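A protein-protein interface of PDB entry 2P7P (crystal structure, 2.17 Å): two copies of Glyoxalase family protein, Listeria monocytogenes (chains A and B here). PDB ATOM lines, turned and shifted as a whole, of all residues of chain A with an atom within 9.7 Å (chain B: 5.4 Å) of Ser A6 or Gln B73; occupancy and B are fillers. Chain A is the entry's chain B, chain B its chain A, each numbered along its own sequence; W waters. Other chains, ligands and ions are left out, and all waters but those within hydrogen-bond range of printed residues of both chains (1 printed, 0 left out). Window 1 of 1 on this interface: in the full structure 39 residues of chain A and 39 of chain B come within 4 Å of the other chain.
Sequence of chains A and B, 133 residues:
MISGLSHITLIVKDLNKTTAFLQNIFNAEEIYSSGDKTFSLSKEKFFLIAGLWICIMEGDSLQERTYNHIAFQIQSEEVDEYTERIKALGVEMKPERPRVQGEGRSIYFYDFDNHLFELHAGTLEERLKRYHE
The backbone carbonyl oxygen of Ala B71 lies within hydrogen-bond range of the backbone NH of Ser A6, 2.8 Å away. The backbone carbonyl oxygen (O) of His A7 is in hydrogen-bond range of the backbone NH (N) of Ala B71 (2.9 Å). O of Gln B73 is in hydrogen-bond range of N of Ser A3, 3.2 Å away. The backbone carbonyl oxygen (O) of Gly A4 is in hydrogen-bond range of the backbone NH (N) of Gln B73, at 2.7 Å. The side-chain amide oxygen of Gln B75 is in hydrogen-bond range of the side-chain hydroxyl of Ser A3 (3.3 Å).
The backbone NH (N) of His B120 is in hydrogen-bond range of the backbone carbonyl oxygen (O) of Phe B72 (2.8 Å). NE2 of Gln B73 is in hydrogen-bond range of O of His B120, 3.4 Å away. The backbone carbonyl oxygen (O) of Gly B122 is in hydrogen-bond range of the side-chain amide nitrogen (NE2) of Gln B73 (2.9 Å). N of Ile B74 sits at hydrogen-bond distance from O of His B120, 3.0 Å away. NE2 of His B120 sits close to N of Gly B122. A ring nitrogen (ND1) of His A7 lies within hydrogen-bond range of the side-chain hydroxyl (OG) of Ser A6 (2.9 Å).
Among the printed residues, merely in contact across the chains: Ser A6 with His B120, Leu A5 with Ala B71, Ile A2 with Gln B73, Gly A4 with Phe B72, Ile A2 with Phe B72, Ser A6 with Gln B73 and Ser A6 with Phe B72.
Printed residues of chain B within 4 Å of Ile A2: Phe B72 (3.6 Å) and Gln B73 (3.5 Å). Printed residues of chain B within 4 Å of Ser A3: Gln B73 and Gln B75. Printed residues of chain B within 4 Å of Gly A4: Phe B72 and Gln B73. Ser A6 touches just these residues of chain B: Ala B71 (2.8 Å), Phe B72 (3.8 Å), Gln B73 (3.8 Å) and His B120 (3.3 Å). Of the printed residues of chain B, His A7 touches Ala B71. Ile A31 touches none of the printed residues of chain B. Of chain A, only Leu A5 (3.3 Å), Ser A6 (2.8 Å) and His A7 (2.9 Å) come within 4 Å of Ala B71. Of the printed residues of chain A, Phe B72 touches Ile A2, Gly A4 and Ser A6. Gln B73 touches just these residues of chain A: Ile A2, Ser A3, Gly A4 and Ser A6. No residue of chain A comes within 4 Å of Ile B74. His B120 touches just one residue of chain A: Ser A6 (3.3 Å). No residue of chain A comes within 4 Å of Gly B122. Thr B123 touches none of the printed residues of chain A. The nearest residue of chain B that does not touch Ser A6 is Gly B122 (4.9 Å). The nearest printed residue of chain B that does not touch His A7 is His B120 (4.1 Å).
Hydrophobic or aromatic side chains of chain A within 4 Å of the printed part of chain B: Ile A2, Leu A5 and His A7. Hydrophobic or aromatic side chains of chain B within 4 Å of the printed part of chain A: Ala B71, Phe B72 and His B120.
No position is printed for both chains. Of the 12 pairs that touch across the chains among the printed residues, none has its exchanged pair printed and touching as well.
Water W1 lies within hydrogen-bond range of OG of Ser A6, OE1 of Gln B73 and O of Gly B122.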
ATOM      1  N   MET A   1     -34.572  -0.643 -29.418  1.00  0.00           N
ATOM      2  CA  MET A   1     -33.746  -1.874 -29.569  1.00  0.00           C
ATOM      3  C   MET A   1     -33.281  -2.408 -28.225  1.00  0.00           C
ATOM      4  O   MET A   1     -33.293  -1.699 -27.221  1.00  0.00           O
ATOM      5  CB  MET A   1     -32.517  -1.594 -30.438  1.00  0.00           C
ATOM      6  CG  MET A   1     -32.814  -1.382 -31.909  1.00  0.00           C
ATOM      7  SD  MET A   1     -31.294  -1.249 -32.884  1.00  0.00           S
ATOM      8  CE  MET A   1     -30.880  -2.994 -33.116  1.00  0.00           C
ATOM      9  N   ILE A   2     -32.866  -3.667 -28.215  1.00  0.00           N
ATOM     10  CA  ILE A   2     -32.389  -4.294 -26.997  1.00  0.00           C
ATOM     11  C   ILE A   2     -30.930  -3.910 -26.777  1.00  0.00           C
ATOM     12  O   ILE A   2     -30.047  -4.358 -27.501  1.00  0.00           O
ATOM     13  CB  ILE A   2     -32.534  -5.827 -27.084  1.00  0.00           C
ATOM     14  CG1 ILE A   2     -34.022  -6.190 -27.134  1.00  0.00           C
ATOM     15  CG2 ILE A   2     -31.847  -6.490 -25.901  1.00  0.00           C
ATOM     16  CD1 ILE A   2     -34.303  -7.668 -27.256  1.00  0.00           C
ATOM     17  N   SER A   3     -30.695  -3.074 -25.769  1.00  0.00           N
ATOM     18  CA  SER A   3     -29.356  -2.594 -25.436  1.00  0.00           C
ATOM     19  C   SER A   3     -28.363  -3.708 -25.167  1.00  0.00           C
ATOM     20  O   SER A   3     -27.172  -3.566 -25.423  1.00  0.00           O
ATOM     21  CB  SER A   3     -29.413  -1.680 -24.210  1.00  0.00           C
ATOM     22  OG  SER A   3     -30.104  -0.477 -24.500  1.00  0.00           O
ATOM     23  N   GLY A   4     -28.851  -4.819 -24.642  1.00  0.00           N
ATOM     24  CA  GLY A   4     -27.961  -5.919 -24.343  1.00  0.00           C
ATOM     25  C   GLY A   4     -28.554  -6.750 -23.236  1.00  0.00           C
ATOM     26  O   GLY A   4     -29.732  -6.624 -22.933  1.00  0.00           O
ATOM     27  N   LEU A   5     -27.735  -7.597 -22.633  1.00  0.00           N
ATOM     28  CA  LEU A   5     -28.189  -8.462 -21.559  1.00  0.00           C
ATOM     29  C   LEU A   5     -28.333  -7.721 -20.239  1.00  0.00           C
ATOM     30  O   LEU A   5     -27.473  -6.927 -19.869  1.00  0.00           O
ATOM     31  CB  LEU A   5     -27.209  -9.617 -21.367  1.00  0.00           C
ATOM     32  CG  LEU A   5     -27.726 -10.724 -20.448  1.00  0.00           C
ATOM     33  CD1 LEU A   5     -28.866 -11.468 -21.145  1.00  0.00           C
ATOM     34  CD2 LEU A   5     -26.595 -11.672 -20.097  1.00  0.00           C
ATOM     35  N   SER A   6     -29.434  -7.978 -19.539  1.00  0.00           N
ATOM     36  CA  SER A   6     -29.667  -7.364 -18.240  1.00  0.00           C
ATOM     37  C   SER A   6     -29.153  -8.308 -17.165  1.00  0.00           C
ATOM     38  O   SER A   6     -28.263  -7.947 -16.400  1.00  0.00           O
ATOM     39  CB  SER A   6     -31.152  -7.106 -18.006  1.00  0.00           C
ATOM     40  OG  SER A   6     -31.376  -6.686 -16.674  1.00  0.00           O
ATOM     41  N   HIS A   7     -29.701  -9.520 -17.116  1.00  0.00           N
ATOM     42  CA  HIS A   7     -29.282 -10.497 -16.117  1.00  0.00           C
ATOM     43  C   HIS A   7     -29.800 -11.911 -16.393  1.00  0.00           C
ATOM     44  O   HIS A   7     -30.540 -12.144 -17.351  1.00  0.00           O
ATOM     45  CB  HIS A   7     -29.769 -10.061 -14.730  1.00  0.00           C
ATOM     46  CG  HIS A   7     -31.263 -10.003 -14.600  1.00  0.00           C
ATOM     47  ND1 HIS A   7     -31.994  -8.866 -14.868  1.00  0.00           N
ATOM     48  CD2 HIS A   7     -32.162 -10.944 -14.223  1.00  0.00           C
ATOM     49  CE1 HIS A   7     -33.277  -9.105 -14.656  1.00  0.00           C
ATOM     50  NE2 HIS A   7     -33.406 -10.360 -14.266  1.00  0.00           N
ATOM     51  N   ILE A   8     -29.404 -12.851 -15.539  1.00  0.00           N
ATOM     52  CA  ILE A   8     -29.838 -14.242 -15.650  1.00  0.00           C
ATOM     53  C   ILE A   8     -30.171 -14.748 -14.249  1.00  0.00           C
ATOM     54  O   ILE A   8     -29.350 -14.669 -13.330  1.00  0.00           O
ATOM     55  CB  ILE A   8     -28.750 -15.132 -16.254  1.00  0.00           C
ATOM     56  CG1 ILE A   8     -28.401 -14.636 -17.659  1.00  0.00           C
ATOM     57  CG2 ILE A   8     -29.238 -16.578 -16.314  1.00  0.00           C
ATOM     58  CD1 ILE A   8     -27.267 -15.399 -18.316  1.00  0.00           C
ATOM     59  N   THR A   9     -31.381 -15.264 -14.090  1.00  0.00           N
ATOM     60  CA  THR A   9     -31.834 -15.758 -12.810  1.00  0.00           C
ATOM     61  C   THR A   9     -32.015 -17.259 -12.846  1.00  0.00           C
ATOM     62  O   THR A   9     -32.658 -17.787 -13.752  1.00  0.00           O
ATOM     63  CB  THR A   9     -33.154 -15.102 -12.437  1.00  0.00           C
ATOM     64  OG1 THR A   9     -32.947 -13.691 -12.283  1.00  0.00           O
ATOM     65  CG2 THR A   9     -33.701 -15.688 -11.148  1.00  0.00           C
ATOM     66  N   ILE A  31     -22.881  -9.577  -4.463  1.00  0.00           N
ATOM     67  CA  ILE A  31     -23.047  -8.130  -4.336  1.00  0.00           C
ATOM     68  C   ILE A  31     -24.374  -7.744  -3.698  1.00  0.00           C
ATOM     69  O   ILE A  31     -24.612  -6.574  -3.398  1.00  0.00           O
ATOM     70  CB  ILE A  31     -23.001  -7.467  -5.718  1.00  0.00           C
ATOM     71  CG1 ILE A  31     -24.130  -8.042  -6.591  1.00  0.00           C
ATOM     72  CG2 ILE A  31     -21.644  -7.709  -6.371  1.00  0.00           C
ATOM     73  CD1 ILE A  31     -24.220  -7.458  -7.988  1.00  0.00           C
ATOM     74  N   PHE A  46     -27.367 -11.801  -5.610  1.00  0.00           N
ATOM     75  CA  PHE A  46     -26.943 -11.316  -6.920  1.00  0.00           C
ATOM     76  C   PHE A  46     -25.436 -11.467  -6.931  1.00  0.00           C
ATOM     77  O   PHE A  46     -24.773 -11.102  -5.961  1.00  0.00           O
ATOM     78  CB  PHE A  46     -27.263  -9.830  -7.116  1.00  0.00           C
ATOM     79  CG  PHE A  46     -28.736  -9.495  -7.128  1.00  0.00           C
ATOM     80  CD1 PHE A  46     -29.143  -8.160  -7.098  1.00  0.00           C
ATOM     81  CD2 PHE A  46     -29.708 -10.493  -7.161  1.00  0.00           C
ATOM     82  CE1 PHE A  46     -30.493  -7.818  -7.096  1.00  0.00           C
ATOM     83  CE2 PHE A  46     -31.070 -10.168  -7.161  1.00  0.00           C
ATOM     84  CZ  PHE A  46     -31.464  -8.825  -7.127  1.00  0.00           C
ATOM     85  N   PHE A  47     -24.890 -12.006  -8.015  1.00  0.00           N
ATOM     86  CA  PHE A  47     -23.451 -12.162  -8.137  1.00  0.00           C
ATOM     87  C   PHE A  47     -22.988 -11.493  -9.413  1.00  0.00           C
ATOM     88  O   PHE A  47     -23.787 -11.199 -10.302  1.00  0.00           O
ATOM     89  CB  PHE A  47     -23.037 -13.630  -8.228  1.00  0.00           C
ATOM     90  CG  PHE A  47     -23.376 -14.452  -7.020  1.00  0.00           C
ATOM     91  CD1 PHE A  47     -24.633 -15.029  -6.884  1.00  0.00           C
ATOM     92  CD2 PHE A  47     -22.416 -14.696  -6.042  1.00  0.00           C
ATOM     93  CE1 PHE A  47     -24.928 -15.846  -5.793  1.00  0.00           C
ATOM     94  CE2 PHE A  47     -22.701 -15.513  -4.942  1.00  0.00           C
ATOM     95  CZ  PHE A  47     -23.958 -16.089  -4.820  1.00  0.00           C
ATOM     96  N   LEU A  48     -21.688 -11.248  -9.487  1.00  0.00           N
ATOM     97  CA  LEU A  48     -21.080 -10.681 -10.674  1.00  0.00           C
ATOM     98  C   LEU A  48     -20.062 -11.713 -11.087  1.00  0.00           C
ATOM     99  O   LEU A  48     -19.249 -12.151 -10.278  1.00  0.00           O
ATOM    100  CB  LEU A  48     -20.376  -9.353 -10.387  1.00  0.00           C
ATOM    101  CG  LEU A  48     -21.240  -8.098 -10.401  1.00  0.00           C
ATOM    102  CD1 LEU A  48     -20.364  -6.862 -10.207  1.00  0.00           C
ATOM    103  CD2 LEU A  48     -21.969  -8.018 -11.735  1.00  0.00           C
ATOM    104  N   GLY A  51     -18.298  -9.686 -15.347  1.00  0.00           N
ATOM    105  CA  GLY A  51     -19.176  -8.606 -15.756  1.00  0.00           C
ATOM    106  C   GLY A  51     -20.666  -8.894 -15.890  1.00  0.00           C
ATOM    107  O   GLY A  51     -21.429  -7.986 -16.185  1.00  0.00           O
ATOM    108  N   LEU A  52     -21.104 -10.127 -15.672  1.00  0.00           N
ATOM    109  CA  LEU A  52     -22.525 -10.426 -15.805  1.00  0.00           C
ATOM    110  C   LEU A  52     -23.282 -10.457 -14.485  1.00  0.00           C
ATOM    111  O   LEU A  52     -22.803 -11.002 -13.495  1.00  0.00           O
ATOM    112  CB  LEU A  52     -22.720 -11.761 -16.516  1.00  0.00           C
ATOM    113  CG  LEU A  52     -22.092 -11.897 -17.898  1.00  0.00           C
ATOM    114  CD1 LEU A  52     -22.392 -13.284 -18.439  1.00  0.00           C
ATOM    115  CD2 LEU A  52     -22.637 -10.822 -18.827  1.00  0.00           C
ATOM    116  N   TRP A  53     -24.475  -9.872 -14.489  1.00  0.00           N
ATOM    117  CA  TRP A  53     -25.338  -9.834 -13.317  1.00  0.00           C
ATOM    118  C   TRP A  53     -26.102 -11.150 -13.241  1.00  0.00           C
ATOM    119  O   TRP A  53     -27.034 -11.376 -14.005  1.00  0.00           O
ATOM    120  CB  TRP A  53     -26.317  -8.656 -13.425  1.00  0.00           C
ATOM    121  CG  TRP A  53     -27.315  -8.560 -12.298  1.00  0.00           C
ATOM    122  CD1 TRP A  53     -27.271  -9.212 -11.095  1.00  0.00           C
ATOM    123  CD2 TRP A  53     -28.503  -7.751 -12.268  1.00  0.00           C
ATOM    124  NE1 TRP A  53     -28.357  -8.861 -10.323  1.00  0.00           N
ATOM    125  CE2 TRP A  53     -29.126  -7.966 -11.017  1.00  0.00           C
ATOM    126  CE3 TRP A  53     -29.100  -6.869 -13.175  1.00  0.00           C
ATOM    127  CZ2 TRP A  53     -30.318  -7.330 -10.653  1.00  0.00           C
ATOM    128  CZ3 TRP A  53     -30.286  -6.236 -12.812  1.00  0.00           C
ATOM    129  CH2 TRP A  53     -30.880  -6.469 -11.563  1.00  0.00           C
ATOM    130  N   ILE A  54     -25.698 -12.015 -12.315  1.00  0.00           N
ATOM    131  CA  ILE A  54     -26.326 -13.318 -12.141  1.00  0.00           C
ATOM    132  C   ILE A  54     -27.101 -13.390 -10.832  1.00  0.00           C
ATOM    133  O   ILE A  54     -26.528 -13.200  -9.766  1.00  0.00           O
ATOM    134  CB  ILE A  54     -25.269 -14.426 -12.124  1.00  0.00           C
ATOM    135  CG1 ILE A  54     -24.317 -14.260 -13.314  1.00  0.00           C
ATOM    136  CG2 ILE A  54     -25.941 -15.778 -12.136  1.00  0.00           C
ATOM    137  CD1 ILE A  54     -25.003 -14.187 -14.656  1.00  0.00           C
ATOM    138  N   CYS A  55     -28.401 -13.673 -10.918  1.00  0.00           N
ATOM    139  CA  CYS A  55     -29.253 -13.771  -9.738  1.00  0.00           C
ATOM    140  C   CYS A  55     -29.590 -15.222  -9.411  1.00  0.00           C
ATOM    141  O   CYS A  55     -29.867 -16.023 -10.297  1.00  0.00           O
ATOM    142  CB  CYS A  55     -30.549 -12.993  -9.952  1.00  0.00           C
ATOM    143  SG  CYS A  55     -30.308 -11.294 -10.535  1.00  0.00           S
ATOM    144  N   ALA B  71     -32.868 -12.369 -19.005  1.00  0.00           N
ATOM    145  CA  ALA B  71     -33.469 -11.048 -19.124  1.00  0.00           C
ATOM    146  C   ALA B  71     -32.633 -10.091 -19.956  1.00  0.00           C
ATOM    147  O   ALA B  71     -31.441  -9.908 -19.702  1.00  0.00           O
ATOM    148  CB  ALA B  71     -33.699 -10.461 -17.743  1.00  0.00           C
ATOM    149  N   PHE B  72     -33.269  -9.474 -20.948  1.00  0.00           N
ATOM    150  CA  PHE B  72     -32.582  -8.521 -21.802  1.00  0.00           C
ATOM    151  C   PHE B  72     -32.955  -7.116 -21.372  1.00  0.00           C
ATOM    152  O   PHE B  72     -34.032  -6.886 -20.822  1.00  0.00           O
ATOM    153  CB  PHE B  72     -32.947  -8.739 -23.275  1.00  0.00           C
ATOM    154  CG  PHE B  72     -32.438 -10.033 -23.840  1.00  0.00           C
ATOM    155  CD1 PHE B  72     -33.161 -11.210 -23.684  1.00  0.00           C
ATOM    156  CD2 PHE B  72     -31.224 -10.079 -24.518  1.00  0.00           C
ATOM    157  CE1 PHE B  72     -32.684 -12.421 -24.196  1.00  0.00           C
ATOM    158  CE2 PHE B  72     -30.738 -11.285 -25.036  1.00  0.00           C
ATOM    159  CZ  PHE B  72     -31.469 -12.454 -24.874  1.00  0.00           C
ATOM    160  N   GLN B  73     -32.058  -6.177 -21.635  1.00  0.00           N
ATOM    161  CA  GLN B  73     -32.260  -4.794 -21.250  1.00  0.00           C
ATOM    162  C   GLN B  73     -33.001  -3.947 -22.278  1.00  0.00           C
ATOM    163  O   GLN B  73     -32.753  -4.044 -23.475  1.00  0.00           O
ATOM    164  CB  GLN B  73     -30.897  -4.162 -20.956  1.00  0.00           C
ATOM    165  CG  GLN B  73     -30.937  -2.691 -20.606  1.00  0.00           C
ATOM    166  CD  GLN B  73     -30.933  -2.448 -19.115  1.00  0.00           C
ATOM    167  OE1 GLN B  73     -29.975  -2.808 -18.421  1.00  0.00           O
ATOM    168  NE2 GLN B  73     -32.004  -1.832 -18.607  1.00  0.00           N
ATOM    169  N   ILE B  74     -33.915  -3.109 -21.796  1.00  0.00           N
ATOM    170  CA  ILE B  74     -34.664  -2.191 -22.651  1.00  0.00           C
ATOM    171  C   ILE B  74     -34.899  -0.931 -21.840  1.00  0.00           C
ATOM    172  O   ILE B  74     -34.601  -0.898 -20.644  1.00  0.00           O
ATOM    173  CB  ILE B  74     -36.041  -2.745 -23.085  1.00  0.00           C
ATOM    174  CG1 ILE B  74     -36.888  -3.076 -21.857  1.00  0.00           C
ATOM    175  CG2 ILE B  74     -35.858  -3.956 -23.972  1.00  0.00           C
ATOM    176  CD1 ILE B  74     -38.356  -3.305 -22.175  1.00  0.00           C
ATOM    177  N   GLN B  75     -35.421   0.106 -22.487  1.00  0.00           N
ATOM    178  CA  GLN B  75     -35.703   1.359 -21.801  1.00  0.00           C
ATOM    179  C   GLN B  75     -37.159   1.303 -21.372  1.00  0.00           C
ATOM    180  O   GLN B  75     -37.955   0.583 -21.978  1.00  0.00           O
ATOM    181  CB  GLN B  75     -35.495   2.558 -22.729  1.00  0.00           C
ATOM    182  CG  GLN B  75     -34.249   2.497 -23.590  1.00  0.00           C
ATOM    183  CD  GLN B  75     -33.100   1.809 -22.898  1.00  0.00           C
ATOM    184  OE1 GLN B  75     -32.909   0.598 -23.041  1.00  0.00           O
ATOM    185  NE2 GLN B  75     -32.330   2.571 -22.130  1.00  0.00           N
ATOM    186  N   HIS B 120     -36.277  -6.224 -19.333  1.00  0.00           N
ATOM    187  CA  HIS B 120     -36.163  -5.427 -18.124  1.00  0.00           C
ATOM    188  C   HIS B 120     -35.774  -3.974 -18.360  1.00  0.00           C
ATOM    189  O   HIS B 120     -34.787  -3.692 -19.037  1.00  0.00           O
ATOM    190  CB  HIS B 120     -35.132  -6.121 -17.225  1.00  0.00           C
ATOM    191  CG  HIS B 120     -34.954  -5.491 -15.882  1.00  0.00           C
ATOM    192  ND1 HIS B 120     -36.004  -5.268 -15.017  1.00  0.00           N
ATOM    193  CD2 HIS B 120     -33.837  -5.083 -15.234  1.00  0.00           C
ATOM    194  CE1 HIS B 120     -35.541  -4.754 -13.891  1.00  0.00           C
ATOM    195  NE2 HIS B 120     -34.229  -4.632 -13.997  1.00  0.00           N
ATOM    196  N   ALA B 121     -36.548  -3.059 -17.781  1.00  0.00           N
ATOM    197  CA  ALA B 121     -36.291  -1.625 -17.919  1.00  0.00           C
ATOM    198  C   ALA B 121     -35.584  -1.020 -16.714  1.00  0.00           C
ATOM    199  O   ALA B 121     -35.505   0.198 -16.592  1.00  0.00           O
ATOM    200  CB  ALA B 121     -37.592  -0.884 -18.161  1.00  0.00           C
ATOM    201  N   GLY B 122     -35.074  -1.853 -15.820  1.00  0.00           N
ATOM    202  CA  GLY B 122     -34.401  -1.312 -14.655  1.00  0.00           C
ATOM    203  C   GLY B 122     -32.905  -1.519 -14.733  1.00  0.00           C
ATOM    204  O   GLY B 122     -32.390  -1.965 -15.766  1.00  0.00           O
ATOM    205  N   THR B 123     -32.206  -1.196 -13.644  1.00  0.00           N
ATOM    206  CA  THR B 123     -30.756  -1.362 -13.580  1.00  0.00           C
ATOM    207  C   THR B 123     -30.341  -1.917 -12.225  1.00  0.00           C
ATOM    208  O   THR B 123     -31.045  -1.753 -11.227  1.00  0.00           O
ATOM    209  CB  THR B 123     -29.998  -0.025 -13.799  1.00  0.00           C
ATOM    210  OG1 THR B 123     -30.378   0.914 -12.786  1.00  0.00           O
ATOM    211  CG2 THR B 123     -30.310   0.555 -15.173  1.00  0.00           C
HETATM  212  O   HOH W   1     -30.631  -4.317 -16.144  1.00  0.00           O
